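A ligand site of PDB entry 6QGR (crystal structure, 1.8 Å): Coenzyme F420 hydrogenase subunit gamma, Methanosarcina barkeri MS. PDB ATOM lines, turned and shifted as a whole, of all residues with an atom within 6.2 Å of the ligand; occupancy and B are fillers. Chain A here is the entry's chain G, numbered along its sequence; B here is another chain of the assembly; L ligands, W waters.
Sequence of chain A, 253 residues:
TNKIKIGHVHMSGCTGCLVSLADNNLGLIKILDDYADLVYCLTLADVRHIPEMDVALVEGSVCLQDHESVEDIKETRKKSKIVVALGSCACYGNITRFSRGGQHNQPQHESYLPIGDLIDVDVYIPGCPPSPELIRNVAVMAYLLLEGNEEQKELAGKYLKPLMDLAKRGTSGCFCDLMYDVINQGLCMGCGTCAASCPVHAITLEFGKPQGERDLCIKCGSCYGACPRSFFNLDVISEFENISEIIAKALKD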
ATOM      1  N   HIS A  10       7.441   9.464  -2.392  1.00  0.00           N
ATOM      2  CA  HIS A  10       6.615   9.341  -3.610  1.00  0.00           C
ATOM      3  C   HIS A  10       7.448   8.799  -4.762  1.00  0.00           C
ATOM      4  O   HIS A  10       8.249   9.523  -5.354  1.00  0.00           O
ATOM      5  CB  HIS A  10       6.020  10.684  -3.974  1.00  0.00           C
ATOM      6  CG  HIS A  10       4.949  10.596  -5.022  1.00  0.00           C
ATOM      7  ND1 HIS A  10       5.235  10.687  -6.371  1.00  0.00           N
ATOM      8  CD2 HIS A  10       3.623  10.380  -4.932  1.00  0.00           C
ATOM      9  CE1 HIS A  10       4.114  10.539  -7.058  1.00  0.00           C
ATOM     10  NE2 HIS A  10       3.128  10.345  -6.204  1.00  0.00           N
ATOM     11  N   SER A  12       6.726   6.010  -8.237  1.00  0.00           N
ATOM     12  CA  SER A  12       5.792   6.089  -9.368  1.00  0.00           C
ATOM     13  C   SER A  12       4.361   5.806  -8.870  1.00  0.00           C
ATOM     14  O   SER A  12       3.818   4.694  -9.018  1.00  0.00           O
ATOM     15  CB  SER A  12       6.216   5.133 -10.476  1.00  0.00           C
ATOM     16  OG  SER A  12       7.288   5.668 -11.241  1.00  0.00           O
ATOM     17  N   GLY A  13       3.813   6.811  -8.186  1.00  0.00           N
ATOM     18  CA  GLY A  13       2.497   6.740  -7.581  1.00  0.00           C
ATOM     19  C   GLY A  13       1.578   7.814  -8.138  1.00  0.00           C
ATOM     20  O   GLY A  13       1.966   8.579  -9.016  1.00  0.00           O
ATOM     21  N   CYS A  14       0.343   7.853  -7.624  1.00  0.00           N
ATOM     22  CA  CYS A  14      -0.621   8.822  -8.145  1.00  0.00           C
ATOM     23  C   CYS A  14      -0.980   9.923  -7.143  1.00  0.00           C
ATOM     24  O   CYS A  14      -1.715  10.859  -7.497  1.00  0.00           O
ATOM     25  CB  CYS A  14      -1.892   8.068  -8.647  1.00  0.00           C
ATOM     26  SG  CYS A  14      -3.111   7.830  -7.356  1.00  0.00           S
ATOM     27  N   THR A  15      -0.466   9.847  -5.910  1.00  0.00           N
ATOM     28  CA  THR A  15      -0.679  10.732  -4.759  1.00  0.00           C
ATOM     29  C   THR A  15      -2.024  10.444  -4.124  1.00  0.00           C
ATOM     30  O   THR A  15      -2.354  11.016  -3.043  1.00  0.00           O
ATOM     31  CB  THR A  15      -0.509  12.224  -5.123  1.00  0.00           C
ATOM     32  OG1 THR A  15       0.725  12.353  -5.829  1.00  0.00           O
ATOM     33  CG2 THR A  15      -0.485  13.164  -3.870  1.00  0.00           C
ATOM     34  N   GLY A  16      -2.826   9.547  -4.719  1.00  0.00           N
ATOM     35  CA  GLY A  16      -4.040   9.080  -4.061  1.00  0.00           C
ATOM     36  C   GLY A  16      -3.796   8.418  -2.718  1.00  0.00           C
ATOM     37  O   GLY A  16      -4.636   8.488  -1.819  1.00  0.00           O
ATOM     38  N   CYS A  17      -2.616   7.794  -2.545  1.00  0.00           N
ATOM     39  CA  CYS A  17      -2.257   7.276  -1.238  1.00  0.00           C
ATOM     40  C   CYS A  17      -2.074   8.405  -0.209  1.00  0.00           C
ATOM     41  O   CYS A  17      -2.607   8.339   0.912  1.00  0.00           O
ATOM     42  CB  CYS A  17      -0.994   6.427  -1.355  1.00  0.00           C
ATOM     43  SG  CYS A  17      -1.428   4.720  -1.943  1.00  0.00           S
ATOM     44  N   LEU A  18      -1.329   9.460  -0.572  1.00  0.00           N
ATOM     45  CA  LEU A  18      -1.236  10.619   0.304  1.00  0.00           C
ATOM     46  C   LEU A  18      -2.604  11.215   0.586  1.00  0.00           C
ATOM     47  O   LEU A  18      -2.934  11.519   1.736  1.00  0.00           O
ATOM     48  CB  LEU A  18      -0.305  11.671  -0.290  1.00  0.00           C
ATOM     49  CG  LEU A  18      -0.123  12.889   0.637  1.00  0.00           C
ATOM     50  CD1 LEU A  18       0.488  12.460   1.981  1.00  0.00           C
ATOM     51  CD2 LEU A  18       0.749  13.973  -0.018  1.00  0.00           C
ATOM     52  N   SER A  20      -5.465   9.732   0.644  1.00  0.00           N
ATOM     53  CA  SER A  20      -6.096   8.855   1.623  1.00  0.00           C
ATOM     54  C   SER A  20      -5.625   9.162   3.046  1.00  0.00           C
ATOM     55  O   SER A  20      -6.439   9.208   3.969  1.00  0.00           O
ATOM     56  CB  SER A  20      -5.821   7.389   1.266  1.00  0.00           C
ATOM     57  OG  SER A  20      -6.306   7.137  -0.053  1.00  0.00           O
ATOM     58  N   GLU A  59       4.782   5.352  -1.321  1.00  0.00           N
ATOM     59  CA  GLU A  59       3.763   5.057  -2.317  1.00  0.00           C
ATOM     60  C   GLU A  59       4.381   4.970  -3.715  1.00  0.00           C
ATOM     61  O   GLU A  59       5.427   5.567  -3.980  1.00  0.00           O
ATOM     62  CB  GLU A  59       2.651   6.116  -2.295  1.00  0.00           C
ATOM     63  CG  GLU A  59       2.971   7.429  -2.943  1.00  0.00           C
ATOM     64  CD  GLU A  59       1.679   8.281  -3.156  1.00  0.00           C
ATOM     65  OE1 GLU A  59       1.178   8.894  -2.194  1.00  0.00           O
ATOM     66  OE2 GLU A  59       1.140   8.252  -4.280  1.00  0.00           O
ATOM     67  N   GLY A  60       3.745   4.179  -4.597  1.00  0.00           N
ATOM     68  CA  GLY A  60       4.216   4.006  -5.944  1.00  0.00           C
ATOM     69  C   GLY A  60       5.223   2.874  -6.086  1.00  0.00           C
ATOM     70  O   GLY A  60       5.830   2.404  -5.121  1.00  0.00           O
ATOM     71  N   LEU A  86       3.031   1.741   1.217  1.00  0.00           N
ATOM     72  CA  LEU A  86       1.719   2.373   1.340  1.00  0.00           C
ATOM     73  C   LEU A  86       0.984   2.241   0.013  1.00  0.00           C
ATOM     74  O   LEU A  86       1.430   2.816  -0.985  1.00  0.00           O
ATOM     75  CB  LEU A  86       1.843   3.864   1.696  1.00  0.00           C
ATOM     76  CG  LEU A  86       0.530   4.625   1.640  1.00  0.00           C
ATOM     77  CD1 LEU A  86      -0.492   4.027   2.590  1.00  0.00           C
ATOM     78  CD2 LEU A  86       0.795   6.096   1.967  1.00  0.00           C
ATOM     79  N   GLY A  87      -0.134   1.515   0.016  1.00  0.00           N
ATOM     80  CA  GLY A  87      -0.952   1.350  -1.183  1.00  0.00           C
ATOM     81  C   GLY A  87      -0.470   0.251  -2.119  1.00  0.00           C
ATOM     82  O   GLY A  87       0.674  -0.219  -2.072  1.00  0.00           O
ATOM     83  N   SER A  88      -1.389  -0.134  -3.032  1.00  0.00           N
ATOM     84  CA  SER A  88      -1.195  -1.308  -3.879  1.00  0.00           C
ATOM     85  C   SER A  88      -0.080  -1.146  -4.910  1.00  0.00           C
ATOM     86  O   SER A  88       0.573  -2.139  -5.249  1.00  0.00           O
ATOM     87  CB  SER A  88      -2.504  -1.682  -4.594  1.00  0.00           C
ATOM     88  OG  SER A  88      -3.489  -2.094  -3.665  1.00  0.00           O
ATOM     89  N   CYS A  89       0.206   0.074  -5.402  1.00  0.00           N
ATOM     90  CA  CYS A  89       1.374   0.208  -6.284  1.00  0.00           C
ATOM     91  C   CYS A  89       2.664  -0.162  -5.550  1.00  0.00           C
ATOM     92  O   CYS A  89       3.497  -0.886  -6.102  1.00  0.00           O
ATOM     93  CB  CYS A  89       1.524   1.641  -6.826  1.00  0.00           C
ATOM     94  SG  CYS A  89       0.169   2.189  -7.962  1.00  0.00           S
ATOM     95  N   ALA A  90       2.858   0.390  -4.334  1.00  0.00           N
ATOM     96  CA  ALA A  90       4.077   0.079  -3.571  1.00  0.00           C
ATOM     97  C   ALA A  90       4.143  -1.418  -3.195  1.00  0.00           C
ATOM     98  O   ALA A  90       5.198  -2.045  -3.338  1.00  0.00           O
ATOM     99  CB  ALA A  90       4.210   0.977  -2.335  1.00  0.00           C
ATOM    100  N   ASN A  94       0.379  -2.993  -9.093  1.00  0.00           N
ATOM    101  CA  ASN A  94      -0.961  -2.426  -9.395  1.00  0.00           C
ATOM    102  C   ASN A  94      -0.975  -2.044 -10.873  1.00  0.00           C
ATOM    103  O   ASN A  94      -0.476  -2.828 -11.720  1.00  0.00           O
ATOM    104  CB  ASN A  94      -1.225  -1.292  -8.391  1.00  0.00           C
ATOM    105  CG  ASN A  94      -2.707  -0.757  -8.403  1.00  0.00           C
ATOM    106  OD1 ASN A  94      -3.664  -1.524  -8.206  1.00  0.00           O
ATOM    107  ND2 ASN A  94      -2.852   0.571  -8.527  1.00  0.00           N
ATOM    108  N   ILE A  95      -1.449  -0.850 -11.252  1.00  0.00           N
ATOM    109  CA  ILE A  95      -1.596  -0.550 -12.677  1.00  0.00           C
ATOM    110  C   ILE A  95      -0.265  -0.503 -13.405  1.00  0.00           C
ATOM    111  O   ILE A  95      -0.246  -0.705 -14.630  1.00  0.00           O
ATOM    112  CB  ILE A  95      -2.386   0.759 -12.896  1.00  0.00           C
ATOM    113  CG1 ILE A  95      -1.701   1.978 -12.213  1.00  0.00           C
ATOM    114  CG2 ILE A  95      -3.885   0.617 -12.431  1.00  0.00           C
ATOM    115  CD1 ILE A  95      -1.693   3.233 -13.164  1.00  0.00           C
ATOM    116  N   GLY A 127      -4.258  -1.736  -0.909  1.00  0.00           N
ATOM    117  CA  GLY A 127      -5.447  -0.971  -1.231  1.00  0.00           C
ATOM    118  C   GLY A 127      -5.169   0.006  -2.348  1.00  0.00           C
ATOM    119  O   GLY A 127      -4.049   0.556  -2.464  1.00  0.00           O
ATOM    120  N   CYS A 128      -6.154   0.162  -3.243  1.00  0.00           N
ATOM    121  CA  CYS A 128      -6.123   1.172  -4.283  1.00  0.00           C
ATOM    122  C   CYS A 128      -7.550   1.693  -4.507  1.00  0.00           C
ATOM    123  O   CYS A 128      -8.320   1.115  -5.280  1.00  0.00           O
ATOM    124  CB  CYS A 128      -5.527   0.625  -5.577  1.00  0.00           C
ATOM    125  SG  CYS A 128      -5.548   1.913  -6.861  1.00  0.00           S
ATOM    126  N   PRO A 129      -7.934   2.780  -3.830  1.00  0.00           N
ATOM    127  CA  PRO A 129      -7.053   3.495  -2.884  1.00  0.00           C
ATOM    128  C   PRO A 129      -7.007   2.787  -1.510  1.00  0.00           C
ATOM    129  O   PRO A 129      -7.977   2.115  -1.128  1.00  0.00           O
ATOM    130  CB  PRO A 129      -7.713   4.880  -2.788  1.00  0.00           C
ATOM    131  CG  PRO A 129      -9.252   4.493  -2.816  1.00  0.00           C
ATOM    132  CD  PRO A 129      -9.317   3.322  -3.825  1.00  0.00           C
ATOM    133  N   PRO A 130      -5.911   2.931  -0.750  1.00  0.00           N
ATOM    134  CA  PRO A 130      -5.875   2.381   0.612  1.00  0.00           C
ATOM    135  C   PRO A 130      -6.889   3.104   1.513  1.00  0.00           C
ATOM    136  O   PRO A 130      -7.178   4.280   1.327  1.00  0.00           O
ATOM    137  CB  PRO A 130      -4.433   2.660   1.067  1.00  0.00           C
ATOM    138  CG  PRO A 130      -4.032   3.934   0.277  1.00  0.00           C
ATOM    139  CD  PRO A 130      -4.717   3.763  -1.078  1.00  0.00           C
ATOM    140  N   ARG B  40       4.753   6.260 -16.922  1.00  0.00           N
ATOM    141  CA  ARG B  40       4.075   4.964 -16.761  1.00  0.00           C
ATOM    142  C   ARG B  40       3.444   4.477 -18.081  1.00  0.00           C
ATOM    143  O   ARG B  40       3.269   3.263 -18.253  1.00  0.00           O
ATOM    144  CB  ARG B  40       3.050   5.057 -15.622  1.00  0.00           C
ATOM    145  CG  ARG B  40       3.726   5.260 -14.212  1.00  0.00           C
ATOM    146  CD  ARG B  40       2.657   5.619 -13.141  1.00  0.00           C
ATOM    147  NE  ARG B  40       2.166   6.984 -13.392  1.00  0.00           N
ATOM    148  CZ  ARG B  40       1.039   7.468 -12.880  1.00  0.00           C
ATOM    149  NH1 ARG B  40       0.310   6.684 -12.065  1.00  0.00           N
ATOM    150  NH2 ARG B  40       0.653   8.718 -13.144  1.00  0.00           N
ATOM    151  N   ARG B  60      -6.070   5.803 -12.318  1.00  0.00           N
ATOM    152  CA  ARG B  60      -4.882   5.689 -11.479  1.00  0.00           C
ATOM    153  C   ARG B  60      -3.711   6.510 -11.991  1.00  0.00           C
ATOM    154  O   ARG B  60      -2.614   6.437 -11.425  1.00  0.00           O
ATOM    155  CB  ARG B  60      -4.490   4.207 -11.310  1.00  0.00           C
ATOM    156  CG  ARG B  60      -5.273   3.506 -10.188  1.00  0.00           C
ATOM    157  CD  ARG B  60      -6.574   2.940 -10.602  1.00  0.00           C
ATOM    158  NE  ARG B  60      -7.288   2.358  -9.458  1.00  0.00           N
ATOM    159  CZ  ARG B  60      -8.579   2.047  -9.451  1.00  0.00           C
ATOM    160  NH1 ARG B  60      -9.292   2.234 -10.564  1.00  0.00           N
ATOM    161  NH2 ARG B  60      -9.162   1.554  -8.353  1.00  0.00           N
ATOM    162  N   VAL B  61      -3.941   7.352 -13.014  1.00  0.00           N
ATOM    163  CA  VAL B  61      -2.960   8.362 -13.350  1.00  0.00           C
ATOM    164  C   VAL B  61      -2.750   9.338 -12.184  1.00  0.00           C
ATOM    165  O   VAL B  61      -1.625   9.790 -11.937  1.00  0.00           O
ATOM    166  CB  VAL B  61      -3.364   9.084 -14.657  1.00  0.00           C
ATOM    167  CG1 VAL B  61      -2.614  10.451 -14.727  1.00  0.00           C
ATOM    168  CG2 VAL B  61      -3.062   8.227 -15.865  1.00  0.00           C
ATOM    169  N   CYS B  62      -3.828   9.650 -11.441  1.00  0.00           N
ATOM    170  CA  CYS B  62      -3.772  10.713 -10.440  1.00  0.00           C
ATOM    171  C   CYS B  62      -4.854  10.523  -9.380  1.00  0.00           C
ATOM    172  O   CYS B  62      -6.030  10.347  -9.713  1.00  0.00           O
ATOM    173  CB  CYS B  62      -3.949  12.092 -11.076  1.00  0.00           C
ATOM    174  SG  CYS B  62      -3.988  13.348  -9.735  1.00  0.00           S
ATOM    175  N   GLY B  63      -4.445  10.601  -8.100  1.00  0.00           N
ATOM    176  CA  GLY B  63      -5.376  10.431  -6.998  1.00  0.00           C
ATOM    177  C   GLY B  63      -6.062  11.698  -6.497  1.00  0.00           C
ATOM    178  O   GLY B  63      -6.912  11.638  -5.597  1.00  0.00           O
ATOM    179  N   ILE B 160     -11.776   8.430  -4.306  1.00  0.00           N
ATOM    180  CA  ILE B 160     -10.532   8.281  -5.053  1.00  0.00           C
ATOM    181  C   ILE B 160     -10.686   7.041  -5.927  1.00  0.00           C
ATOM    182  O   ILE B 160     -10.814   5.938  -5.405  1.00  0.00           O
ATOM    183  CB  ILE B 160      -9.324   8.146  -4.103  1.00  0.00           C
ATOM    184  CG1 ILE B 160      -9.399   9.238  -3.001  1.00  0.00           C
ATOM    185  CG2 ILE B 160      -8.043   8.143  -4.859  1.00  0.00           C
ATOM    186  CD1 ILE B 160      -8.315   9.129  -1.945  1.00  0.00           C
ATOM    187  N   HIS B 161     -10.653   7.230  -7.276  1.00  0.00           N
ATOM    188  CA  HIS B 161     -10.906   6.182  -8.268  1.00  0.00           C
ATOM    189  C   HIS B 161     -12.378   5.751  -8.217  1.00  0.00           C
ATOM    190  O   HIS B 161     -12.715   4.642  -7.776  1.00  0.00           O
ATOM    191  CB  HIS B 161      -9.914   5.024  -8.086  1.00  0.00           C
ATOM    192  CG  HIS B 161      -8.484   5.480  -7.981  1.00  0.00           C
ATOM    193  ND1 HIS B 161      -7.912   6.368  -8.871  1.00  0.00           N
ATOM    194  CD2 HIS B 161      -7.521   5.193  -7.056  1.00  0.00           C
ATOM    195  CE1 HIS B 161      -6.662   6.607  -8.500  1.00  0.00           C
ATOM    196  NE2 HIS B 161      -6.389   5.886  -7.424  1.00  0.00           N
HETATM  197 FE1  LIG L   1      -2.585   5.771  -6.554  1.00  0.00          FE
HETATM  198 FE2  LIG L   1      -1.091   3.431  -6.655  1.00  0.00          FE
HETATM  199 FE3  LIG L   1      -3.815   3.372  -6.161  1.00  0.00          FE
HETATM  200 FE4  LIG L   1      -2.070   4.527  -4.167  1.00  0.00          FE
HETATM  201  S1  LIG L   1      -2.055   2.369  -4.775  1.00  0.00           S
HETATM  202  S2  LIG L   1      -4.195   5.375  -5.013  1.00  0.00           S
HETATM  203  S3  LIG L   1      -0.384   5.424  -5.632  1.00  0.00           S
HETATM  204  S4  LIG L   1      -2.868   4.150  -8.197  1.00  0.00           S
HETATM  205  O   HOH W   1       1.068   2.843  -3.731  1.00  0.00           O
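The backbone NH (N) of Cys 89 lies close to a sulfur (S1) of the ligand, at 3.3 Å. The side-chain sulfur of Cys 89 is bound to an iron atom (FE2) of the ligand, 2.2 Å away. The backbone NH of Cys 14 sits close to a sulfur (S3) of the ligand (3.2 Å). FE1 of the ligand is bound by SG of Cys 14 (2.3 Å). The backbone NH (N) of Cys 17 sits close to a sulfur (S2) of the ligand, at 3.8 Å. An iron atom (FE4) of the ligand is bound by the side-chain sulfur (SG) of Cys 17, 2.3 Å away. The side-chain sulfur of Cys 128 binds an iron atom (FE3) of the ligand (2.4 Å). The backbone NH (N) of Ser 88 lies close to a sulfur (S1) of the ligand (3.1 Å). A sulfur (S2) of the ligand sits close to a ring nitrogen (NE2) of His 161 of chain B, 3.3 Å away. ND2 of Asn 94 sits close to S4 of the ligand (3.6 Å).
The side-chain sulfur (SG) of Cys 89 lies close to the side-chain amide nitrogen (ND2) of Asn 94 (3.5 Å). N of Gly 16 lies close to SG of Cys 14 (3.2 Å). The backbone NH (N) of Gly 63 of chain B is in hydrogen-bond range of the backbone carbonyl oxygen (O) of Cys 14. The side-chain sulfur (SG) of Cys 17 sits close to the backbone carbonyl oxygen (O) of Leu 86 (3.6 Å). O of Cys 128 sits at hydrogen-bond distance from NH2 of Arg 60 of chain B. N of Ser 88 sits at hydrogen-bond distance from O of Gly 127 (2.8 Å). N of Leu 18 is in hydrogen-bond range of OE1 of Glu 59 (3.0 Å). The side-chain hydroxyl (OG) of Ser 20 is in hydrogen-bond range of the backbone carbonyl oxygen (O) of Gly 16 (2.8 Å).
The side-chain carboxylate of Glu 59 sits close to a sulfur (S3) of the ligand, 3.5 Å away. The backbone carbonyl oxygen (O) of Gly 127 sits close to a sulfur (S1) of the ligand (3.6 Å). CA of Gly 13 touches S3 of the ligand, 3.7 Å away. CA of Gly 16 touches S2 of the ligand, 3.8 Å away. Gly 87 touches the ligand. CG of Arg 60 of chain B touches S4 of the ligand (3.2 Å). The nearest printed residue that does not touch the ligand is Pro 129 (4.03 Å).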
